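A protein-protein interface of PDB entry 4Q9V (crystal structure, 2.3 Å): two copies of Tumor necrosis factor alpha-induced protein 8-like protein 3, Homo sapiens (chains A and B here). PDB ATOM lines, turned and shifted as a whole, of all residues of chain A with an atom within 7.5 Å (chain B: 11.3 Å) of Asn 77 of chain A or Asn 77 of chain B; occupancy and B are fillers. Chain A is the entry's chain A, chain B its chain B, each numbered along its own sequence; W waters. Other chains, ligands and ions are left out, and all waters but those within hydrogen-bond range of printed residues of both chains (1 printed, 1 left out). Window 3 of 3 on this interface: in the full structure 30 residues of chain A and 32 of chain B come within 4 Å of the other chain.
The backbone carbonyl oxygen (O) of Asn 76 of chain B sits close to the backbone carbonyl oxygen (O) of Asn 76 of chain A, 3.1 Å away. O of Asn 76 of chain B lies close to ND2 of Asn 77 of chain A (3.5 Å). O of Asn 77 of chain B lies within hydrogen-bond range of ND2 of Asn 77 of chain A, at 3.1 Å.
The backbone carbonyl oxygen (O) of Gln 78 of chain B is in hydrogen-bond range of a ring nitrogen (NE2) of His 134 of chain B (3.2 Å). The backbone carbonyl oxygen (O) of Leu 73 of chain B lies within hydrogen-bond range of the backbone NH (N) of Gln 78 of chain B, at 2.9 Å.
NH2 of Arg 75 of chain A touches NE2 of Gln 78 of chain B (3.7 Å). Asn 77 of chain A touches Gln 78 of chain B (ND2 to CA, 3.9 Å).
Of chain B, only Asn 76 (3.3 Å), Asn 77 (3.1 Å) and Gln 78 (3.9 Å) come within 4 Å of Asn 77 of chain A. Of chain A, only Asn 77 (3.1 Å) comes within 4 Å of Asn 77 of chain B. No residue of chain B comes within 4 Å of Tyr 74 of chain A. Asn 76 of chain A touches just one residue of chain B: Asn 76. No residue of chain B comes within 4 Å of Gln 78 of chain A. Of the printed residues of chain A, Gln 78 of chain B touches Arg 75 and Asn 77. Printed residues of chain B within 4 Å of Arg 75 of chain A: Gln 78. Printed residues of chain A within 4 Å of Asn 76 of chain B: Asn 76 (3.1 Å) and Asn 77 (3.3 Å). Tyr 74 of chain B touches none of the printed residues of chain A. Arg 133 of chain B touches none of the printed residues of chain A. The nearest residue of chain A that does not touch Asn 77 of chain B is Asn 76 of chain A (4.8 Å).
Of the 23 printed residues of chain B, 3 touch a printed residue of chain A. Of the 12 printed residues of chain A, 3 touch a printed residue of chain B. Among the printed residues, 5 pairs touch across the chains. Among the printed residues, no Asp or Glu carboxylate lies within 4 Å of a Lys or Arg side-chain nitrogen of the other chain.
Arg 75 of chain A touches Gln 78 of chain B, but with the chains exchanged Gln 78 of chain A does not touch Arg 75 of chain B (5.0 Å). Asn 76 of chain B touches its own counterpart, Asn 76 of chain A. Asn 77 of chain A touches Asn 76 of chain B, but with the chains exchanged Asn 76 of chain A does not touch Asn 77 of chain B (4.8 Å). Asn 77 of chain A touches Gln 78 of chain B, but with the chains exchanged Gln 78 of chain A does not touch Asn 77 of chain B (5.3 Å). Of the 5 pairs that touch across the chains among the printed residues, 2 have their exchanged pair printed and touching as well.
Water W1 bridges the guanidinium group of Arg 75 of chain A (2.6 Å) and the side-chain amide nitrogen of Gln 78 of chain B (3.2 Å).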
ATOM      1  N   GLY A  71      -8.167 -10.881  -9.260  1.00  0.00           N
ATOM      2  CA  GLY A  71      -6.734 -11.144  -9.279  1.00  0.00           C
ATOM      3  C   GLY A  71      -5.954  -9.899  -8.870  1.00  0.00           C
ATOM      4  O   GLY A  71      -5.010  -9.962  -8.089  1.00  0.00           O
ATOM      5  N   ILE A  72      -6.379  -8.748  -9.369  1.00  0.00           N
ATOM      6  CA  ILE A  72      -5.670  -7.506  -9.091  1.00  0.00           C
ATOM      7  C   ILE A  72      -5.887  -7.049  -7.656  1.00  0.00           C
ATOM      8  O   ILE A  72      -4.934  -6.615  -7.014  1.00  0.00           O
ATOM      9  CB  ILE A  72      -6.017  -6.402 -10.139  1.00  0.00           C
ATOM     10  CG1 ILE A  72      -5.424  -6.781 -11.498  1.00  0.00           C
ATOM     11  CG2 ILE A  72      -5.463  -5.039  -9.737  1.00  0.00           C
ATOM     12  CD1 ILE A  72      -5.856  -5.859 -12.626  1.00  0.00           C
ATOM     13  N   LEU A  73      -7.123  -7.135  -7.158  1.00  0.00           N
ATOM     14  CA  LEU A  73      -7.368  -6.846  -5.742  1.00  0.00           C
ATOM     15  C   LEU A  73      -6.466  -7.741  -4.872  1.00  0.00           C
ATOM     16  O   LEU A  73      -5.882  -7.303  -3.877  1.00  0.00           O
ATOM     17  CB  LEU A  73      -8.845  -7.065  -5.399  1.00  0.00           C
ATOM     18  CG  LEU A  73      -9.836  -6.009  -5.902  1.00  0.00           C
ATOM     19  CD1 LEU A  73     -11.257  -6.506  -5.809  1.00  0.00           C
ATOM     20  CD2 LEU A  73      -9.696  -4.708  -5.112  1.00  0.00           C
ATOM     21  N   TYR A  74      -6.342  -9.002  -5.263  1.00  0.00           N
ATOM     22  CA  TYR A  74      -5.521  -9.939  -4.507  1.00  0.00           C
ATOM     23  C   TYR A  74      -4.030  -9.569  -4.524  1.00  0.00           C
ATOM     24  O   TYR A  74      -3.433  -9.388  -3.465  1.00  0.00           O
ATOM     25  CB  TYR A  74      -5.748 -11.377  -4.986  1.00  0.00           C
ATOM     26  CG  TYR A  74      -5.154 -12.416  -4.055  1.00  0.00           C
ATOM     27  CD1 TYR A  74      -5.837 -12.833  -2.918  1.00  0.00           C
ATOM     28  CD2 TYR A  74      -3.906 -12.979  -4.310  1.00  0.00           C
ATOM     29  CE1 TYR A  74      -5.292 -13.787  -2.055  1.00  0.00           C
ATOM     30  CE2 TYR A  74      -3.354 -13.919  -3.453  1.00  0.00           C
ATOM     31  CZ  TYR A  74      -4.050 -14.321  -2.330  1.00  0.00           C
ATOM     32  OH  TYR A  74      -3.488 -15.258  -1.487  1.00  0.00           O
ATOM     33  N   ARG A  75      -3.431  -9.434  -5.707  1.00  0.00           N
ATOM     34  CA  ARG A  75      -1.995  -9.198  -5.763  1.00  0.00           C
ATOM     35  C   ARG A  75      -1.630  -7.880  -5.111  1.00  0.00           C
ATOM     36  O   ARG A  75      -0.571  -7.764  -4.512  1.00  0.00           O
ATOM     37  CB  ARG A  75      -1.446  -9.228  -7.198  1.00  0.00           C
ATOM     38  CG  ARG A  75      -0.193 -10.109  -7.340  1.00  0.00           C
ATOM     39  CD  ARG A  75       1.098  -9.318  -7.590  1.00  0.00           C
ATOM     40  NE  ARG A  75       1.369  -8.356  -6.527  1.00  0.00           N
ATOM     41  CZ  ARG A  75       2.502  -7.671  -6.384  1.00  0.00           C
ATOM     42  NH1 ARG A  75       3.513  -7.825  -7.235  1.00  0.00           N
ATOM     43  NH2 ARG A  75       2.613  -6.820  -5.377  1.00  0.00           N
ATOM     44  N   ASN A  76      -2.511  -6.894  -5.212  1.00  0.00           N
ATOM     45  CA  ASN A  76      -2.199  -5.575  -4.687  1.00  0.00           C
ATOM     46  C   ASN A  76      -2.522  -5.433  -3.200  1.00  0.00           C
ATOM     47  O   ASN A  76      -2.428  -4.344  -2.664  1.00  0.00           O
ATOM     48  CB  ASN A  76      -2.925  -4.482  -5.484  1.00  0.00           C
ATOM     49  CG  ASN A  76      -2.319  -4.257  -6.861  1.00  0.00           C
ATOM     50  OD1 ASN A  76      -1.360  -4.927  -7.257  1.00  0.00           O
ATOM     51  ND2 ASN A  76      -2.890  -3.317  -7.605  1.00  0.00           N
ATOM     52  N   ASN A  77      -2.895  -6.537  -2.556  1.00  0.00           N
ATOM     53  CA  ASN A  77      -3.306  -6.528  -1.153  1.00  0.00           C
ATOM     54  C   ASN A  77      -4.383  -5.520  -0.857  1.00  0.00           C
ATOM     55  O   ASN A  77      -4.300  -4.798   0.119  1.00  0.00           O
ATOM     56  CB  ASN A  77      -2.101  -6.319  -0.212  1.00  0.00           C
ATOM     57  CG  ASN A  77      -1.192  -7.528  -0.193  1.00  0.00           C
ATOM     58  OD1 ASN A  77      -1.657  -8.652  -0.371  1.00  0.00           O
ATOM     59  ND2 ASN A  77       0.101  -7.308  -0.012  1.00  0.00           N
ATOM     60  N   GLN A  78      -5.408  -5.492  -1.698  1.00  0.00           N
ATOM     61  CA  GLN A  78      -6.512  -4.562  -1.537  1.00  0.00           C
ATOM     62  C   GLN A  78      -7.623  -5.143  -0.666  1.00  0.00           C
ATOM     63  O   GLN A  78      -8.605  -4.466  -0.377  1.00  0.00           O
ATOM     64  CB  GLN A  78      -7.077  -4.179  -2.905  1.00  0.00           C
ATOM     65  CG  GLN A  78      -7.300  -2.691  -3.095  1.00  0.00           C
ATOM     66  CD  GLN A  78      -6.012  -1.943  -3.367  1.00  0.00           C
ATOM     67  OE1 GLN A  78      -5.058  -2.028  -2.596  1.00  0.00           O
ATOM     68  NE2 GLN A  78      -5.979  -1.206  -4.470  1.00  0.00           N
ATOM     69  N   PHE A  79      -7.467  -6.397  -0.256  1.00  0.00           N
ATOM     70  CA  PHE A  79      -8.500  -7.059   0.537  1.00  0.00           C
ATOM     71  C   PHE A  79      -8.251  -6.866   2.046  1.00  0.00           C
ATOM     72  O   PHE A  79      -7.131  -7.089   2.528  1.00  0.00           O
ATOM     73  CB  PHE A  79      -8.521  -8.556   0.225  1.00  0.00           C
ATOM     74  CG  PHE A  79      -9.179  -8.919  -1.088  1.00  0.00           C
ATOM     75  CD1 PHE A  79     -10.423  -8.396  -1.440  1.00  0.00           C
ATOM     76  CD2 PHE A  79      -8.543  -9.810  -1.972  1.00  0.00           C
ATOM     77  CE1 PHE A  79     -11.040  -8.764  -2.661  1.00  0.00           C
ATOM     78  CE2 PHE A  79      -9.138 -10.190  -3.174  1.00  0.00           C
ATOM     79  CZ  PHE A  79     -10.396  -9.670  -3.524  1.00  0.00           C
ATOM     80  N   SER A  80      -9.290  -6.473   2.789  1.00  0.00           N
ATOM     81  CA  SER A  80      -9.202  -6.366   4.256  1.00  0.00           C
ATOM     82  C   SER A  80      -9.111  -7.757   4.870  1.00  0.00           C
ATOM     83  O   SER A  80      -9.265  -8.755   4.171  1.00  0.00           O
ATOM     84  CB  SER A  80     -10.445  -5.667   4.813  1.00  0.00           C
ATOM     85  OG  SER A  80     -11.591  -6.481   4.600  1.00  0.00           O
ATOM     86  N   LEU A  84     -10.042 -11.269   3.299  1.00  0.00           N
ATOM     87  CA  LEU A  84      -9.114 -12.398   3.168  1.00  0.00           C
ATOM     88  C   LEU A  84      -9.734 -13.723   3.699  1.00  0.00           C
ATOM     89  O   LEU A  84      -9.570 -14.806   3.091  1.00  0.00           O
ATOM     90  CB  LEU A  84      -7.769 -12.046   3.830  1.00  0.00           C
ATOM     91  CG  LEU A  84      -6.959 -11.034   3.022  1.00  0.00           C
ATOM     92  CD1 LEU A  84      -5.643 -10.651   3.706  1.00  0.00           C
ATOM     93  CD2 LEU A  84      -6.684 -11.594   1.655  1.00  0.00           C
ATOM     94  N   HIS A 134     -15.795  -3.375  -3.311  1.00  0.00           N
ATOM     95  CA  HIS A 134     -14.857  -2.944  -4.345  1.00  0.00           C
ATOM     96  C   HIS A 134     -15.560  -2.914  -5.683  1.00  0.00           C
ATOM     97  O   HIS A 134     -14.945  -3.114  -6.720  1.00  0.00           O
ATOM     98  CB  HIS A 134     -13.670  -3.899  -4.400  1.00  0.00           C
ATOM     99  CG  HIS A 134     -12.982  -4.083  -3.082  1.00  0.00           C
ATOM    100  ND1 HIS A 134     -11.956  -3.270  -2.655  1.00  0.00           N
ATOM    101  CD2 HIS A 134     -13.162  -5.004  -2.098  1.00  0.00           C
ATOM    102  CE1 HIS A 134     -11.533  -3.677  -1.469  1.00  0.00           C
ATOM    103  NE2 HIS A 134     -12.253  -4.726  -1.112  1.00  0.00           N
ATOM    104  N   LEU B  30       3.836   9.194  -6.458  1.00  0.00           N
ATOM    105  CA  LEU B  30       4.568   8.916  -5.224  1.00  0.00           C
ATOM    106  C   LEU B  30       5.582  10.020  -4.902  1.00  0.00           C
ATOM    107  O   LEU B  30       5.941  10.234  -3.742  1.00  0.00           O
ATOM    108  CB  LEU B  30       5.283   7.571  -5.330  1.00  0.00           C
ATOM    109  CG  LEU B  30       4.353   6.370  -5.396  1.00  0.00           C
ATOM    110  CD1 LEU B  30       5.072   5.145  -5.995  1.00  0.00           C
ATOM    111  CD2 LEU B  30       3.818   6.095  -3.992  1.00  0.00           C
ATOM    112  N   ILE B  68      10.543   4.789  -5.793  1.00  0.00           N
ATOM    113  CA  ILE B  68       9.269   4.351  -6.362  1.00  0.00           C
ATOM    114  C   ILE B  68       8.922   2.939  -5.891  1.00  0.00           C
ATOM    115  O   ILE B  68       7.775   2.635  -5.582  1.00  0.00           O
ATOM    116  CB  ILE B  68       9.308   4.396  -7.893  1.00  0.00           C
ATOM    117  CG1 ILE B  68       9.335   5.845  -8.371  1.00  0.00           C
ATOM    118  CG2 ILE B  68       8.093   3.696  -8.487  1.00  0.00           C
ATOM    119  CD1 ILE B  68       8.013   6.553  -8.147  1.00  0.00           C
ATOM    120  N   LYS B  69       9.940   2.089  -5.809  1.00  0.00           N
ATOM    121  CA  LYS B  69       9.765   0.735  -5.304  1.00  0.00           C
ATOM    122  C   LYS B  69       9.233   0.749  -3.876  1.00  0.00           C
ATOM    123  O   LYS B  69       8.279   0.044  -3.556  1.00  0.00           O
ATOM    124  CB  LYS B  69      11.087  -0.028  -5.364  1.00  0.00           C
ATOM    125  CG  LYS B  69      10.993  -1.464  -4.884  1.00  0.00           C
ATOM    126  CD  LYS B  69      11.864  -2.383  -5.723  1.00  0.00           C
ATOM    127  CE  LYS B  69      12.763  -3.241  -4.848  1.00  0.00           C
ATOM    128  NZ  LYS B  69      12.066  -4.468  -4.375  1.00  0.00           N
ATOM    129  N   ILE B  70       9.851   1.554  -3.019  1.00  0.00           N
ATOM    130  CA  ILE B  70       9.421   1.665  -1.623  1.00  0.00           C
ATOM    131  C   ILE B  70       7.997   2.199  -1.541  1.00  0.00           C
ATOM    132  O   ILE B  70       7.164   1.653  -0.803  1.00  0.00           O
ATOM    133  CB  ILE B  70      10.381   2.551  -0.786  1.00  0.00           C
ATOM    134  CG1 ILE B  70      11.739   1.854  -0.618  1.00  0.00           C
ATOM    135  CG2 ILE B  70       9.790   2.874   0.601  1.00  0.00           C
ATOM    136  CD1 ILE B  70      12.785   2.725   0.123  1.00  0.00           C
ATOM    137  N   GLY B  71       7.721   3.248  -2.314  1.00  0.00           N
ATOM    138  CA  GLY B  71       6.401   3.868  -2.339  1.00  0.00           C
ATOM    139  C   GLY B  71       5.324   2.883  -2.763  1.00  0.00           C
ATOM    140  O   GLY B  71       4.228   2.838  -2.199  1.00  0.00           O
ATOM    141  N   ILE B  72       5.641   2.064  -3.755  1.00  0.00           N
ATOM    142  CA  ILE B  72       4.679   1.092  -4.259  1.00  0.00           C
ATOM    143  C   ILE B  72       4.425  -0.021  -3.234  1.00  0.00           C
ATOM    144  O   ILE B  72       3.261  -0.352  -2.959  1.00  0.00           O
ATOM    145  CB  ILE B  72       5.094   0.547  -5.646  1.00  0.00           C
ATOM    146  CG1 ILE B  72       4.713   1.564  -6.724  1.00  0.00           C
ATOM    147  CG2 ILE B  72       4.392  -0.776  -5.934  1.00  0.00           C
ATOM    148  CD1 ILE B  72       5.448   1.383  -8.038  1.00  0.00           C
ATOM    149  N   LEU B  73       5.498  -0.575  -2.659  1.00  0.00           N
ATOM    150  CA  LEU B  73       5.350  -1.509  -1.537  1.00  0.00           C
ATOM    151  C   LEU B  73       4.461  -0.936  -0.433  1.00  0.00           C
ATOM    152  O   LEU B  73       3.564  -1.624   0.045  1.00  0.00           O
ATOM    153  CB  LEU B  73       6.710  -1.934  -0.963  1.00  0.00           C
ATOM    154  CG  LEU B  73       7.668  -2.718  -1.864  1.00  0.00           C
ATOM    155  CD1 LEU B  73       9.032  -2.977  -1.191  1.00  0.00           C
ATOM    156  CD2 LEU B  73       7.032  -4.030  -2.315  1.00  0.00           C
ATOM    157  N   TYR B  74       4.692   0.323  -0.044  1.00  0.00           N
ATOM    158  CA  TYR B  74       3.939   0.932   1.062  1.00  0.00           C
ATOM    159  C   TYR B  74       2.478   1.211   0.703  1.00  0.00           C
ATOM    160  O   TYR B  74       1.589   1.102   1.552  1.00  0.00           O
ATOM    161  CB  TYR B  74       4.617   2.231   1.541  1.00  0.00           C
ATOM    162  CG  TYR B  74       3.867   2.978   2.643  1.00  0.00           C
ATOM    163  CD1 TYR B  74       4.125   2.729   3.990  1.00  0.00           C
ATOM    164  CD2 TYR B  74       2.928   3.952   2.334  1.00  0.00           C
ATOM    165  CE1 TYR B  74       3.449   3.418   4.992  1.00  0.00           C
ATOM    166  CE2 TYR B  74       2.248   4.642   3.323  1.00  0.00           C
ATOM    167  CZ  TYR B  74       2.511   4.373   4.649  1.00  0.00           C
ATOM    168  OH  TYR B  74       1.835   5.066   5.630  1.00  0.00           O
ATOM    169  N   ARG B  75       2.241   1.605  -0.546  1.00  0.00           N
ATOM    170  CA  ARG B  75       0.888   1.874  -1.035  1.00  0.00           C
ATOM    171  C   ARG B  75       0.097   0.555  -1.214  1.00  0.00           C
ATOM    172  O   ARG B  75      -1.086   0.475  -0.869  1.00  0.00           O
ATOM    173  CB  ARG B  75       0.935   2.704  -2.336  1.00  0.00           C
ATOM    174  CG  ARG B  75      -0.436   3.113  -2.894  1.00  0.00           C
ATOM    175  CD  ARG B  75      -0.326   3.989  -4.164  1.00  0.00           C
ATOM    176  NE  ARG B  75       0.277   5.299  -3.896  1.00  0.00           N
ATOM    177  CZ  ARG B  75       0.311   6.313  -4.764  1.00  0.00           C
ATOM    178  NH1 ARG B  75      -0.229   6.187  -5.972  1.00  0.00           N
ATOM    179  NH2 ARG B  75       0.880   7.465  -4.419  1.00  0.00           N
ATOM    180  N   ASN B  76       0.762  -0.487  -1.711  1.00  0.00           N
ATOM    181  CA  ASN B  76       0.126  -1.798  -1.873  1.00  0.00           C
ATOM    182  C   ASN B  76       0.205  -2.727  -0.674  1.00  0.00           C
ATOM    183  O   ASN B  76       0.092  -3.950  -0.832  1.00  0.00           O
ATOM    184  CB  ASN B  76       0.715  -2.519  -3.090  1.00  0.00           C
ATOM    185  CG  ASN B  76       0.227  -1.937  -4.380  1.00  0.00           C
ATOM    186  OD1 ASN B  76      -0.760  -1.192  -4.400  1.00  0.00           O
ATOM    187  ND2 ASN B  76       0.911  -2.256  -5.473  1.00  0.00           N
ATOM    188  N   ASN B  77       0.409  -2.150   0.510  1.00  0.00           N
ATOM    189  CA  ASN B  77       0.544  -2.914   1.751  1.00  0.00           C
ATOM    190  C   ASN B  77       1.347  -4.206   1.667  1.00  0.00           C
ATOM    191  O   ASN B  77       0.934  -5.237   2.196  1.00  0.00           O
ATOM    192  CB  ASN B  77      -0.835  -3.179   2.353  1.00  0.00           C
ATOM    193  CG  ASN B  77      -1.515  -1.909   2.777  1.00  0.00           C
ATOM    194  OD1 ASN B  77      -1.320  -1.425   3.896  1.00  0.00           O
ATOM    195  ND2 ASN B  77      -2.306  -1.342   1.877  1.00  0.00           N
ATOM    196  N   GLN B  78       2.489  -4.150   0.994  1.00  0.00           N
ATOM    197  CA  GLN B  78       3.375  -5.302   0.883  1.00  0.00           C
ATOM    198  C   GLN B  78       4.227  -5.488   2.148  1.00  0.00           C
ATOM    199  O   GLN B  78       4.829  -6.549   2.357  1.00  0.00           O
ATOM    200  CB  GLN B  78       4.275  -5.165  -0.359  1.00  0.00           C
ATOM    201  CG  GLN B  78       3.687  -5.720  -1.662  1.00  0.00           C
ATOM    202  CD  GLN B  78       4.409  -6.981  -2.137  1.00  0.00           C
ATOM    203  OE1 GLN B  78       4.056  -8.092  -1.742  1.00  0.00           O
ATOM    204  NE2 GLN B  78       5.432  -6.809  -2.981  1.00  0.00           N
ATOM    205  N   PHE B  79       4.268  -4.451   2.989  1.00  0.00           N
ATOM    206  CA  PHE B  79       5.083  -4.455   4.205  1.00  0.00           C
ATOM    207  C   PHE B  79       4.424  -5.182   5.366  1.00  0.00           C
ATOM    208  O   PHE B  79       3.290  -4.869   5.734  1.00  0.00           O
ATOM    209  CB  PHE B  79       5.408  -3.013   4.640  1.00  0.00           C
ATOM    210  CG  PHE B  79       6.458  -2.338   3.791  1.00  0.00           C
ATOM    211  CD1 PHE B  79       7.632  -3.007   3.459  1.00  0.00           C
ATOM    212  CD2 PHE B  79       6.262  -1.054   3.313  1.00  0.00           C
ATOM    213  CE1 PHE B  79       8.603  -2.402   2.668  1.00  0.00           C
ATOM    214  CE2 PHE B  79       7.222  -0.431   2.522  1.00  0.00           C
ATOM    215  CZ  PHE B  79       8.397  -1.107   2.200  1.00  0.00           C
ATOM    216  N   SER B  80       5.154  -6.129   5.951  1.00  0.00           N
ATOM    217  CA  SER B  80       4.725  -6.833   7.158  1.00  0.00           C
ATOM    218  C   SER B  80       4.761  -5.902   8.364  1.00  0.00           C
ATOM    219  O   SER B  80       5.133  -4.744   8.237  1.00  0.00           O
ATOM    220  CB  SER B  80       5.667  -7.992   7.437  1.00  0.00           C
ATOM    221  OG  SER B  80       6.957  -7.506   7.757  1.00  0.00           O
ATOM    222  N   GLN B  81       4.386  -6.415   9.537  1.00  0.00           N
ATOM    223  CA  GLN B  81       4.393  -5.620  10.771  1.00  0.00           C
ATOM    224  C   GLN B  81       5.801  -5.154  11.160  1.00  0.00           C
ATOM    225  O   GLN B  81       6.029  -3.964  11.456  1.00  0.00           O
ATOM    226  CB  GLN B  81       3.752  -6.407  11.914  1.00  0.00           C
ATOM    227  N   GLU B  82       6.734  -6.104  11.171  1.00  0.00           N
ATOM    228  CA  GLU B  82       8.140  -5.819  11.436  1.00  0.00           C
ATOM    229  C   GLU B  82       8.617  -4.739  10.463  1.00  0.00           C
ATOM    230  O   GLU B  82       9.224  -3.720  10.856  1.00  0.00           O
ATOM    231  CB  GLU B  82       8.973  -7.104  11.257  1.00  0.00           C
ATOM    232  CG  GLU B  82      10.135  -7.281  12.254  1.00  0.00           C
ATOM    233  CD  GLU B  82      11.268  -6.264  12.074  1.00  0.00           C
ATOM    234  OE1 GLU B  82      11.113  -5.093  12.513  1.00  0.00           O
ATOM    235  OE2 GLU B  82      12.322  -6.647  11.506  1.00  0.00           O
ATOM    236  N   GLU B  83       8.305  -4.959   9.189  1.00  0.00           N
ATOM    237  CA  GLU B  83       8.718  -4.045   8.140  1.00  0.00           C
ATOM    238  C   GLU B  83       8.099  -2.666   8.303  1.00  0.00           C
ATOM    239  O   GLU B  83       8.735  -1.677   7.992  1.00  0.00           O
ATOM    240  CB  GLU B  83       8.415  -4.634   6.757  1.00  0.00           C
ATOM    241  CG  GLU B  83       9.328  -5.805   6.385  1.00  0.00           C
ATOM    242  CD  GLU B  83       8.853  -6.547   5.149  1.00  0.00           C
ATOM    243  OE1 GLU B  83       7.775  -6.190   4.617  1.00  0.00           O
ATOM    244  OE2 GLU B  83       9.564  -7.477   4.711  1.00  0.00           O
ATOM    245  N   LEU B  84       6.864  -2.596   8.788  1.00  0.00           N
ATOM    246  CA  LEU B  84       6.251  -1.296   9.046  1.00  0.00           C
ATOM    247  C   LEU B  84       6.945  -0.580  10.206  1.00  0.00           C
ATOM    248  O   LEU B  84       7.069   0.659  10.208  1.00  0.00           O
ATOM    249  CB  LEU B  84       4.750  -1.441   9.299  1.00  0.00           C
ATOM    250  CG  LEU B  84       3.932  -1.700   8.033  1.00  0.00           C
ATOM    251  CD1 LEU B  84       2.501  -2.080   8.389  1.00  0.00           C
ATOM    252  CD2 LEU B  84       3.958  -0.484   7.123  1.00  0.00           C
ATOM    253  N   VAL B  87       9.701   0.913   8.638  1.00  0.00           N
ATOM    254  CA  VAL B  87       9.254   2.070   7.871  1.00  0.00           C
ATOM    255  C   VAL B  87       9.210   3.284   8.791  1.00  0.00           C
ATOM    256  O   VAL B  87       9.612   4.371   8.396  1.00  0.00           O
ATOM    257  CB  VAL B  87       7.864   1.849   7.193  1.00  0.00           C
ATOM    258  CG1 VAL B  87       7.316   3.159   6.614  1.00  0.00           C
ATOM    259  CG2 VAL B  87       7.950   0.796   6.100  1.00  0.00           C
ATOM    260  N   ARG B  91      11.352   6.677   8.695  1.00  0.00           N
ATOM    261  CA  ARG B  91      10.720   7.999   8.688  1.00  0.00           C
ATOM    262  C   ARG B  91      11.457   8.944   9.650  1.00  0.00           C
ATOM    263  O   ARG B  91      11.808  10.085   9.309  1.00  0.00           O
ATOM    264  CB  ARG B  91       9.248   7.887   9.107  1.00  0.00           C
ATOM    265  CG  ARG B  91       8.275   7.707   7.957  1.00  0.00           C
ATOM    266  CD  ARG B  91       6.841   7.998   8.395  1.00  0.00           C
ATOM    267  NE  ARG B  91       6.048   8.524   7.288  1.00  0.00           N
ATOM    268  CZ  ARG B  91       5.177   7.812   6.579  1.00  0.00           C
ATOM    269  NH1 ARG B  91       4.971   6.537   6.866  1.00  0.00           N
ATOM    270  NH2 ARG B  91       4.503   8.377   5.584  1.00  0.00           N
ATOM    271  N   LEU B 130      14.495  -2.641   4.664  1.00  0.00           N
ATOM    272  CA  LEU B 130      13.141  -2.451   4.159  1.00  0.00           C
ATOM    273  C   LEU B 130      12.856  -3.364   2.975  1.00  0.00           C
ATOM    274  O   LEU B 130      11.764  -3.952   2.885  1.00  0.00           O
ATOM    275  CB  LEU B 130      12.949  -0.997   3.737  1.00  0.00           C
ATOM    276  CG  LEU B 130      11.652  -0.315   4.134  1.00  0.00           C
ATOM    277  CD1 LEU B 130      11.073  -0.953   5.389  1.00  0.00           C
ATOM    278  CD2 LEU B 130      11.901   1.181   4.345  1.00  0.00           C
ATOM    279  N   ARG B 133      13.102  -8.535   2.069  1.00  0.00           N
ATOM    280  CA  ARG B 133      12.104  -9.536   1.684  1.00  0.00           C
ATOM    281  C   ARG B 133      11.394  -9.193   0.377  1.00  0.00           C
ATOM    282  O   ARG B 133      10.377  -9.805   0.033  1.00  0.00           O
ATOM    283  CB  ARG B 133      11.057  -9.712   2.796  1.00  0.00           C
ATOM    284  CG  ARG B 133      11.568 -10.429   4.034  1.00  0.00           C
ATOM    285  CD  ARG B 133      10.466 -10.598   5.091  1.00  0.00           C
ATOM    286  NE  ARG B 133      10.870 -11.519   6.158  1.00  0.00           N
ATOM    287  CZ  ARG B 133      11.336 -11.149   7.350  1.00  0.00           C
ATOM    288  NH1 ARG B 133      11.452  -9.858   7.661  1.00  0.00           N
ATOM    289  NH2 ARG B 133      11.677 -12.074   8.240  1.00  0.00           N
ATOM    290  N   HIS B 134      11.922  -8.224  -0.359  1.00  0.00           N
ATOM    291  CA  HIS B 134      11.250  -7.762  -1.558  1.00  0.00           C
ATOM    292  C   HIS B 134      12.231  -7.405  -2.656  1.00  0.00           C
ATOM    293  O   HIS B 134      11.877  -6.667  -3.578  1.00  0.00           O
ATOM    294  CB  HIS B 134      10.411  -6.526  -1.252  1.00  0.00           C
ATOM    295  CG  HIS B 134       9.219  -6.787  -0.383  1.00  0.00           C
ATOM    296  ND1 HIS B 134       8.021  -7.262  -0.880  1.00  0.00           N
ATOM    297  CD2 HIS B 134       9.046  -6.671   0.955  1.00  0.00           C
ATOM    298  CE1 HIS B 134       7.167  -7.425   0.112  1.00  0.00           C
ATOM    299  NE2 HIS B 134       7.762  -7.070   1.236  1.00  0.00           N
HETATM  300  O   HOH W   1       4.128  -4.739  -5.110  1.00  0.00           O
